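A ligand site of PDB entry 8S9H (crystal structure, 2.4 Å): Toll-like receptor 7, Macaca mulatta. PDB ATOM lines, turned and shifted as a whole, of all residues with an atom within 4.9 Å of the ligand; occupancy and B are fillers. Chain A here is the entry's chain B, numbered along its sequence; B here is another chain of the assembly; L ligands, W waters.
The side-chain carboxylate of Asp 533 of chain B sits at hydrogen-bond distance from a nitrogen (N6) of the ligand (2.5 Å).
The backbone carbonyl oxygen (O) of Thr 564 of chain B lies within hydrogen-bond range of a nitrogen (N6) of the ligand (2.9 Å).
The side-chain hydroxyl of Tyr 242 sits at hydrogen-bond distance from an oxygen (O3) of the ligand.
NE2 of Gln 332 lies within hydrogen-bond range of O3 of the ligand, at 3.0 Å.
An oxygen (O3) of the ligand is in hydrogen-bond range of the backbone carbonyl oxygen (O) of Leu 331, 3.0 Å away.
The side-chain amino group of Lys 410 is in salt-bridge range of the side-chain carboxylate of Asp 533 of chain B (3.4 Å).
The side-chain hydroxyl of Tyr 242 lies within hydrogen-bond range of the side-chain hydroxyl of Thr 564 of chain B, 3.2 Å away.
OG1 of Thr 564 of chain B is in hydrogen-bond range of ND2 of Asn 243.
The backbone carbonyl oxygen of Phe 386 sits at hydrogen-bond distance from the side-chain hydroxyl of Tyr 334.
Merely in contact with the ligand: Val 359, Ile 563 of chain B, Tyr 334, Phe 386, Leu 535 of chain B, Val 333, Phe 329, Thr 510 of chain B, Gly 562 of chain B and Glu 330.
Of the 20 residues printed, 15 come within 4 Å of the ligand.
Along chain A the residues within 4 Å of the ligand span positions 242 to 386.
Water W1 lies within hydrogen-bond range of an oxygen (O3) of the ligand, the side-chain amide nitrogen (NE2) of Gln 332 and the side-chain hydroxyl (OH) of Tyr 242.
Water W3 lies within hydrogen-bond range of OD1 of Asp 533 of chain B (2.7 Å), O of Thr 564 of chain B (3.2 Å) and N6 of the ligand (3.5 Å).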
ATOM      1  N   TYR A 242     -12.203  38.812 -19.486  1.00  0.00           N
ATOM      2  CA  TYR A 242     -12.461  37.860 -20.561  1.00  0.00           C
ATOM      3  C   TYR A 242     -13.932  37.945 -20.989  1.00  0.00           C
ATOM      4  O   TYR A 242     -14.816  37.765 -20.156  1.00  0.00           O
ATOM      5  CB  TYR A 242     -12.081  36.432 -20.156  1.00  0.00           C
ATOM      6  CG  TYR A 242     -11.986  35.486 -21.332  1.00  0.00           C
ATOM      7  CD1 TYR A 242     -10.959  35.600 -22.262  1.00  0.00           C
ATOM      8  CD2 TYR A 242     -12.932  34.495 -21.534  1.00  0.00           C
ATOM      9  CE1 TYR A 242     -10.892  34.774 -23.365  1.00  0.00           C
ATOM     10  CE2 TYR A 242     -12.861  33.630 -22.616  1.00  0.00           C
ATOM     11  CZ  TYR A 242     -11.842  33.781 -23.545  1.00  0.00           C
ATOM     12  OH  TYR A 242     -11.744  32.947 -24.627  1.00  0.00           O
ATOM     13  N   ASN A 243     -14.163  38.264 -22.281  1.00  0.00           N
ATOM     14  CA  ASN A 243     -15.490  38.437 -22.889  1.00  0.00           C
ATOM     15  C   ASN A 243     -16.326  39.530 -22.214  1.00  0.00           C
ATOM     16  O   ASN A 243     -17.549  39.394 -22.125  1.00  0.00           O
ATOM     17  CB  ASN A 243     -16.269  37.119 -22.985  1.00  0.00           C
ATOM     18  CG  ASN A 243     -15.661  36.127 -23.940  1.00  0.00           C
ATOM     19  OD1 ASN A 243     -15.022  36.490 -24.937  1.00  0.00           O
ATOM     20  ND2 ASN A 243     -15.886  34.850 -23.695  1.00  0.00           N
ATOM     21  N   PHE A 327     -18.816  32.035 -13.135  1.00  0.00           N
ATOM     22  CA  PHE A 327     -17.759  32.430 -14.059  1.00  0.00           C
ATOM     23  C   PHE A 327     -16.398  32.569 -13.392  1.00  0.00           C
ATOM     24  O   PHE A 327     -15.776  33.634 -13.434  1.00  0.00           O
ATOM     25  CB  PHE A 327     -18.178  33.686 -14.830  1.00  0.00           C
ATOM     26  CG  PHE A 327     -19.408  33.437 -15.675  1.00  0.00           C
ATOM     27  CD1 PHE A 327     -19.314  32.761 -16.882  1.00  0.00           C
ATOM     28  CD2 PHE A 327     -20.664  33.803 -15.230  1.00  0.00           C
ATOM     29  CE1 PHE A 327     -20.455  32.477 -17.632  1.00  0.00           C
ATOM     30  CE2 PHE A 327     -21.799  33.526 -15.982  1.00  0.00           C
ATOM     31  CZ  PHE A 327     -21.685  32.874 -17.186  1.00  0.00           C
ATOM     32  N   PHE A 329     -14.108  29.914 -14.125  1.00  0.00           N
ATOM     33  CA  PHE A 329     -13.339  28.953 -14.923  1.00  0.00           C
ATOM     34  C   PHE A 329     -11.947  29.432 -15.315  1.00  0.00           C
ATOM     35  O   PHE A 329     -11.716  30.630 -15.445  1.00  0.00           O
ATOM     36  CB  PHE A 329     -14.126  28.583 -16.207  1.00  0.00           C
ATOM     37  CG  PHE A 329     -14.250  29.670 -17.256  1.00  0.00           C
ATOM     38  CD1 PHE A 329     -15.282  30.595 -17.195  1.00  0.00           C
ATOM     39  CD2 PHE A 329     -13.404  29.716 -18.340  1.00  0.00           C
ATOM     40  CE1 PHE A 329     -15.401  31.578 -18.165  1.00  0.00           C
ATOM     41  CE2 PHE A 329     -13.522  30.702 -19.301  1.00  0.00           C
ATOM     42  CZ  PHE A 329     -14.531  31.629 -19.211  1.00  0.00           C
ATOM     43  N   GLU A 330     -11.028  28.483 -15.547  1.00  0.00           N
ATOM     44  CA  GLU A 330      -9.685  28.812 -16.019  1.00  0.00           C
ATOM     45  C   GLU A 330      -9.880  29.026 -17.525  1.00  0.00           C
ATOM     46  O   GLU A 330     -10.396  28.125 -18.199  1.00  0.00           O
ATOM     47  CB  GLU A 330      -8.700  27.655 -15.775  1.00  0.00           C
ATOM     48  CG  GLU A 330      -8.474  27.299 -14.316  1.00  0.00           C
ATOM     49  CD  GLU A 330      -7.694  26.018 -14.128  1.00  0.00           C
ATOM     50  OE1 GLU A 330      -8.268  25.053 -13.576  1.00  0.00           O
ATOM     51  OE2 GLU A 330      -6.515  25.966 -14.558  1.00  0.00           O
ATOM     52  N   LEU A 331      -9.504  30.201 -18.034  1.00  0.00           N
ATOM     53  CA  LEU A 331      -9.755  30.618 -19.424  1.00  0.00           C
ATOM     54  C   LEU A 331      -9.568  29.531 -20.518  1.00  0.00           C
ATOM     55  O   LEU A 331     -10.349  29.520 -21.472  1.00  0.00           O
ATOM     56  CB  LEU A 331      -8.911  31.863 -19.822  1.00  0.00           C
ATOM     57  CG  LEU A 331      -8.978  33.140 -18.954  1.00  0.00           C
ATOM     58  CD1 LEU A 331      -8.292  34.300 -19.660  1.00  0.00           C
ATOM     59  CD2 LEU A 331     -10.420  33.539 -18.586  1.00  0.00           C
ATOM     60  N   GLN A 332      -8.557  28.641 -20.410  1.00  0.00           N
ATOM     61  CA  GLN A 332      -8.318  27.625 -21.443  1.00  0.00           C
ATOM     62  C   GLN A 332      -8.281  26.177 -20.913  1.00  0.00           C
ATOM     63  O   GLN A 332      -7.454  25.390 -21.369  1.00  0.00           O
ATOM     64  CB  GLN A 332      -7.016  27.966 -22.196  1.00  0.00           C
ATOM     65  CG  GLN A 332      -7.088  29.239 -23.050  1.00  0.00           C
ATOM     66  CD  GLN A 332      -7.861  29.024 -24.334  1.00  0.00           C
ATOM     67  OE1 GLN A 332      -7.318  28.550 -25.339  1.00  0.00           O
ATOM     68  NE2 GLN A 332      -9.150  29.363 -24.346  1.00  0.00           N
ATOM     69  N   VAL A 333      -9.206  25.808 -20.006  1.00  0.00           N
ATOM     70  CA  VAL A 333      -9.286  24.441 -19.468  1.00  0.00           C
ATOM     71  C   VAL A 333     -10.752  24.009 -19.468  1.00  0.00           C
ATOM     72  O   VAL A 333     -11.577  24.662 -18.821  1.00  0.00           O
ATOM     73  CB  VAL A 333      -8.704  24.308 -18.035  1.00  0.00           C
ATOM     74  CG1 VAL A 333      -8.708  22.847 -17.571  1.00  0.00           C
ATOM     75  CG2 VAL A 333      -7.308  24.912 -17.920  1.00  0.00           C
ATOM     76  N   TYR A 334     -11.073  22.901 -20.143  1.00  0.00           N
ATOM     77  CA  TYR A 334     -12.419  22.343 -20.150  1.00  0.00           C
ATOM     78  C   TYR A 334     -12.357  21.136 -19.209  1.00  0.00           C
ATOM     79  O   TYR A 334     -12.038  20.029 -19.633  1.00  0.00           O
ATOM     80  CB  TYR A 334     -12.835  21.944 -21.589  1.00  0.00           C
ATOM     81  CG  TYR A 334     -14.282  21.550 -21.839  1.00  0.00           C
ATOM     82  CD1 TYR A 334     -15.255  21.722 -20.865  1.00  0.00           C
ATOM     83  CD2 TYR A 334     -14.692  21.085 -23.084  1.00  0.00           C
ATOM     84  CE1 TYR A 334     -16.584  21.419 -21.107  1.00  0.00           C
ATOM     85  CE2 TYR A 334     -16.014  20.759 -23.331  1.00  0.00           C
ATOM     86  CZ  TYR A 334     -16.964  20.928 -22.348  1.00  0.00           C
ATOM     87  OH  TYR A 334     -18.280  20.607 -22.607  1.00  0.00           O
ATOM     88  N   VAL A 359     -17.554  25.449 -16.038  1.00  0.00           N
ATOM     89  CA  VAL A 359     -17.115  24.783 -17.274  1.00  0.00           C
ATOM     90  C   VAL A 359     -16.549  23.395 -16.988  1.00  0.00           C
ATOM     91  O   VAL A 359     -15.385  23.255 -16.604  1.00  0.00           O
ATOM     92  CB  VAL A 359     -16.160  25.658 -18.132  1.00  0.00           C
ATOM     93  CG1 VAL A 359     -15.827  24.977 -19.449  1.00  0.00           C
ATOM     94  CG2 VAL A 359     -16.773  27.041 -18.392  1.00  0.00           C
ATOM     95  N   THR A 384     -24.849  27.581 -17.893  1.00  0.00           N
ATOM     96  CA  THR A 384     -23.690  28.007 -18.698  1.00  0.00           C
ATOM     97  C   THR A 384     -22.385  27.277 -18.313  1.00  0.00           C
ATOM     98  O   THR A 384     -21.379  27.908 -18.020  1.00  0.00           O
ATOM     99  CB  THR A 384     -23.547  29.561 -18.679  1.00  0.00           C
ATOM    100  OG1 THR A 384     -24.845  30.161 -18.812  1.00  0.00           O
ATOM    101  CG2 THR A 384     -22.649  30.094 -19.794  1.00  0.00           C
ATOM    102  N   PHE A 386     -21.564  24.025 -20.122  1.00  0.00           N
ATOM    103  CA  PHE A 386     -21.224  23.142 -21.231  1.00  0.00           C
ATOM    104  C   PHE A 386     -21.112  21.683 -20.735  1.00  0.00           C
ATOM    105  O   PHE A 386     -20.182  20.981 -21.117  1.00  0.00           O
ATOM    106  CB  PHE A 386     -19.964  23.619 -21.985  1.00  0.00           C
ATOM    107  CG  PHE A 386     -20.149  24.968 -22.633  1.00  0.00           C
ATOM    108  CD1 PHE A 386     -20.755  25.077 -23.871  1.00  0.00           C
ATOM    109  CD2 PHE A 386     -19.774  26.133 -21.977  1.00  0.00           C
ATOM    110  CE1 PHE A 386     -20.978  26.318 -24.445  1.00  0.00           C
ATOM    111  CE2 PHE A 386     -19.992  27.378 -22.563  1.00  0.00           C
ATOM    112  CZ  PHE A 386     -20.582  27.461 -23.795  1.00  0.00           C
ATOM    113  N   LYS A 410     -24.720  21.380 -22.773  1.00  0.00           N
ATOM    114  CA  LYS A 410     -24.636  20.445 -23.900  1.00  0.00           C
ATOM    115  C   LYS A 410     -25.166  19.028 -23.573  1.00  0.00           C
ATOM    116  O   LYS A 410     -24.769  18.075 -24.242  1.00  0.00           O
ATOM    117  CB  LYS A 410     -23.156  20.323 -24.345  1.00  0.00           C
ATOM    118  CG  LYS A 410     -22.506  21.636 -24.819  1.00  0.00           C
ATOM    119  CD  LYS A 410     -22.744  21.930 -26.291  1.00  0.00           C
ATOM    120  CE  LYS A 410     -21.781  22.946 -26.834  1.00  0.00           C
ATOM    121  NZ  LYS A 410     -21.958  23.158 -28.299  1.00  0.00           N
ATOM    122  N   THR B 510     -18.872  22.693 -32.015  1.00  0.00           N
ATOM    123  CA  THR B 510     -17.778  23.658 -32.067  1.00  0.00           C
ATOM    124  C   THR B 510     -16.879  23.199 -33.218  1.00  0.00           C
ATOM    125  O   THR B 510     -16.039  22.326 -33.028  1.00  0.00           O
ATOM    126  CB  THR B 510     -16.997  23.658 -30.736  1.00  0.00           C
ATOM    127  OG1 THR B 510     -16.669  22.316 -30.382  1.00  0.00           O
ATOM    128  CG2 THR B 510     -17.780  24.308 -29.614  1.00  0.00           C
ATOM    129  N   ASP B 533     -21.375  27.162 -33.277  1.00  0.00           N
ATOM    130  CA  ASP B 533     -20.652  27.625 -32.097  1.00  0.00           C
ATOM    131  C   ASP B 533     -19.229  27.991 -32.533  1.00  0.00           C
ATOM    132  O   ASP B 533     -18.413  27.108 -32.764  1.00  0.00           O
ATOM    133  CB  ASP B 533     -20.653  26.521 -31.023  1.00  0.00           C
ATOM    134  CG  ASP B 533     -20.252  26.985 -29.641  1.00  0.00           C
ATOM    135  OD1 ASP B 533     -19.683  28.095 -29.526  1.00  0.00           O
ATOM    136  OD2 ASP B 533     -20.493  26.232 -28.674  1.00  0.00           O
ATOM    137  N   LEU B 534     -18.940  29.302 -32.667  1.00  0.00           N
ATOM    138  CA  LEU B 534     -17.620  29.772 -33.071  1.00  0.00           C
ATOM    139  C   LEU B 534     -16.685  29.883 -31.865  1.00  0.00           C
ATOM    140  O   LEU B 534     -16.262  30.977 -31.495  1.00  0.00           O
ATOM    141  CB  LEU B 534     -17.693  31.105 -33.837  1.00  0.00           C
ATOM    142  CG  LEU B 534     -18.343  31.075 -35.232  1.00  0.00           C
ATOM    143  CD1 LEU B 534     -18.741  32.473 -35.690  1.00  0.00           C
ATOM    144  CD2 LEU B 534     -17.420  30.448 -36.278  1.00  0.00           C
ATOM    145  N   LEU B 535     -16.350  28.748 -31.255  1.00  0.00           N
ATOM    146  CA  LEU B 535     -15.389  28.700 -30.154  1.00  0.00           C
ATOM    147  C   LEU B 535     -13.985  28.832 -30.754  1.00  0.00           C
ATOM    148  O   LEU B 535     -13.171  29.588 -30.241  1.00  0.00           O
ATOM    149  CB  LEU B 535     -15.527  27.374 -29.363  1.00  0.00           C
ATOM    150  CG  LEU B 535     -14.392  26.994 -28.404  1.00  0.00           C
ATOM    151  CD1 LEU B 535     -14.206  28.024 -27.293  1.00  0.00           C
ATOM    152  CD2 LEU B 535     -14.644  25.626 -27.801  1.00  0.00           C
ATOM    153  N   GLY B 562     -21.593  35.607 -21.962  1.00  0.00           N
ATOM    154  CA  GLY B 562     -20.329  34.982 -21.581  1.00  0.00           C
ATOM    155  C   GLY B 562     -19.762  33.908 -22.480  1.00  0.00           C
ATOM    156  O   GLY B 562     -18.701  33.375 -22.170  1.00  0.00           O
ATOM    157  N   ILE B 563     -20.437  33.592 -23.589  1.00  0.00           N
ATOM    158  CA  ILE B 563     -19.981  32.554 -24.509  1.00  0.00           C
ATOM    159  C   ILE B 563     -18.983  33.162 -25.506  1.00  0.00           C
ATOM    160  O   ILE B 563     -19.274  34.202 -26.073  1.00  0.00           O
ATOM    161  CB  ILE B 563     -21.212  31.887 -25.190  1.00  0.00           C
ATOM    162  CG1 ILE B 563     -22.062  31.139 -24.125  1.00  0.00           C
ATOM    163  CG2 ILE B 563     -20.766  30.951 -26.334  1.00  0.00           C
ATOM    164  CD1 ILE B 563     -23.271  30.379 -24.607  1.00  0.00           C
ATOM    165  N   THR B 564     -17.826  32.526 -25.695  1.00  0.00           N
ATOM    166  CA  THR B 564     -16.795  32.996 -26.638  1.00  0.00           C
ATOM    167  C   THR B 564     -17.289  32.876 -28.083  1.00  0.00           C
ATOM    168  O   THR B 564     -17.806  31.826 -28.457  1.00  0.00           O
ATOM    169  CB  THR B 564     -15.487  32.193 -26.420  1.00  0.00           C
ATOM    170  OG1 THR B 564     -14.922  32.549 -25.157  1.00  0.00           O
ATOM    171  CG2 THR B 564     -14.451  32.427 -27.507  1.00  0.00           C
HETATM  172  N1  LIG L   1     -17.167  28.660 -25.750  1.00  0.00           N
HETATM  173  C1  LIG L   1     -14.615  24.953 -23.388  1.00  0.00           C
HETATM  174  C2  LIG L   1     -13.602  25.671 -22.734  1.00  0.00           C
HETATM  175  N2  LIG L   1     -18.345  26.932 -26.941  1.00  0.00           N
HETATM  176  C3  LIG L   1     -12.285  25.548 -23.166  1.00  0.00           C
HETATM  177  O1  LIG L   1     -14.052  26.472 -21.710  1.00  0.00           O
HETATM  178  C4  LIG L   1     -17.948  28.208 -26.763  1.00  0.00           C
HETATM  179  C5  LIG L   1     -18.106  24.630 -25.866  1.00  0.00           C
HETATM  180  C6  LIG L   1     -16.077  25.022 -23.013  1.00  0.00           C
HETATM  181  N3  LIG L   1     -16.870  25.231 -24.212  1.00  0.00           N
HETATM  182  C7  LIG L   1     -17.888  26.054 -26.025  1.00  0.00           C
HETATM  183  C8  LIG L   1     -17.079  26.386 -24.920  1.00  0.00           C
HETATM  184  O2  LIG L   1      -4.279  24.312 -27.813  1.00  0.00           O
HETATM  185  C9  LIG L   1     -16.753  27.761 -24.846  1.00  0.00           C
HETATM  186  N4  LIG L   1     -17.491  24.161 -24.802  1.00  0.00           N
HETATM  187  C10 LIG L   1     -11.992  24.696 -24.227  1.00  0.00           C
HETATM  188  C11 LIG L   1     -13.057  24.023 -24.806  1.00  0.00           C
HETATM  189  N5  LIG L   1     -14.327  24.134 -24.406  1.00  0.00           N
HETATM  190  C12 LIG L   1     -10.587  24.504 -24.751  1.00  0.00           C
HETATM  191  N6  LIG L   1     -18.348  29.108 -27.668  1.00  0.00           N
HETATM  192  N7  LIG L   1     -15.957  28.187 -23.828  1.00  0.00           N
HETATM  193  C13 LIG L   1     -13.084  27.056 -20.830  1.00  0.00           C
HETATM  194  C14 LIG L   1     -15.660  29.585 -23.519  1.00  0.00           C
HETATM  195  C15 LIG L   1     -16.689  30.182 -22.561  1.00  0.00           C
HETATM  196  C16 LIG L   1     -17.113  29.299 -21.399  1.00  0.00           C
HETATM  197  C17 LIG L   1     -18.092  29.978 -20.478  1.00  0.00           C
HETATM  198  C18 LIG L   1     -14.210  29.746 -23.040  1.00  0.00           C
HETATM  199  C19 LIG L   1     -13.175  29.430 -24.105  1.00  0.00           C
HETATM  200  O3  LIG L   1     -11.984  30.166 -23.906  1.00  0.00           O
HETATM  201  C20 LIG L   1      -9.556  24.050 -23.713  1.00  0.00           C
HETATM  202  C21 LIG L   1      -8.238  23.710 -24.409  1.00  0.00           C
HETATM  203  N8  LIG L   1      -7.686  24.841 -25.190  1.00  0.00           N
HETATM  204  C22 LIG L   1      -8.685  25.377 -26.149  1.00  0.00           C
HETATM  205  C23 LIG L   1     -10.021  25.719 -25.494  1.00  0.00           C
HETATM  206  C24 LIG L   1      -6.299  24.667 -25.749  1.00  0.00           C
HETATM  207  C25 LIG L   1      -5.740  25.824 -26.600  1.00  0.00           C
HETATM  208  C26 LIG L   1      -4.334  25.534 -27.077  1.00  0.00           C
HETATM  209  C27 LIG L   1      -4.651  23.195 -26.998  1.00  0.00           C
HETATM  210  C28 LIG L   1      -6.068  23.328 -26.478  1.00  0.00           C
HETATM  211  O   HOH W   1     -10.772  30.510 -26.468  1.00  0.00           O
HETATM  212  O   HOH W   2      -9.556  27.105 -29.025  1.00  0.00           O
HETATM  213  O   HOH W   3     -20.129  30.600 -30.276  1.00  0.00           O
HETATM  214  O   HOH W   4     -15.263  22.084 -26.556  1.00  0.00           O
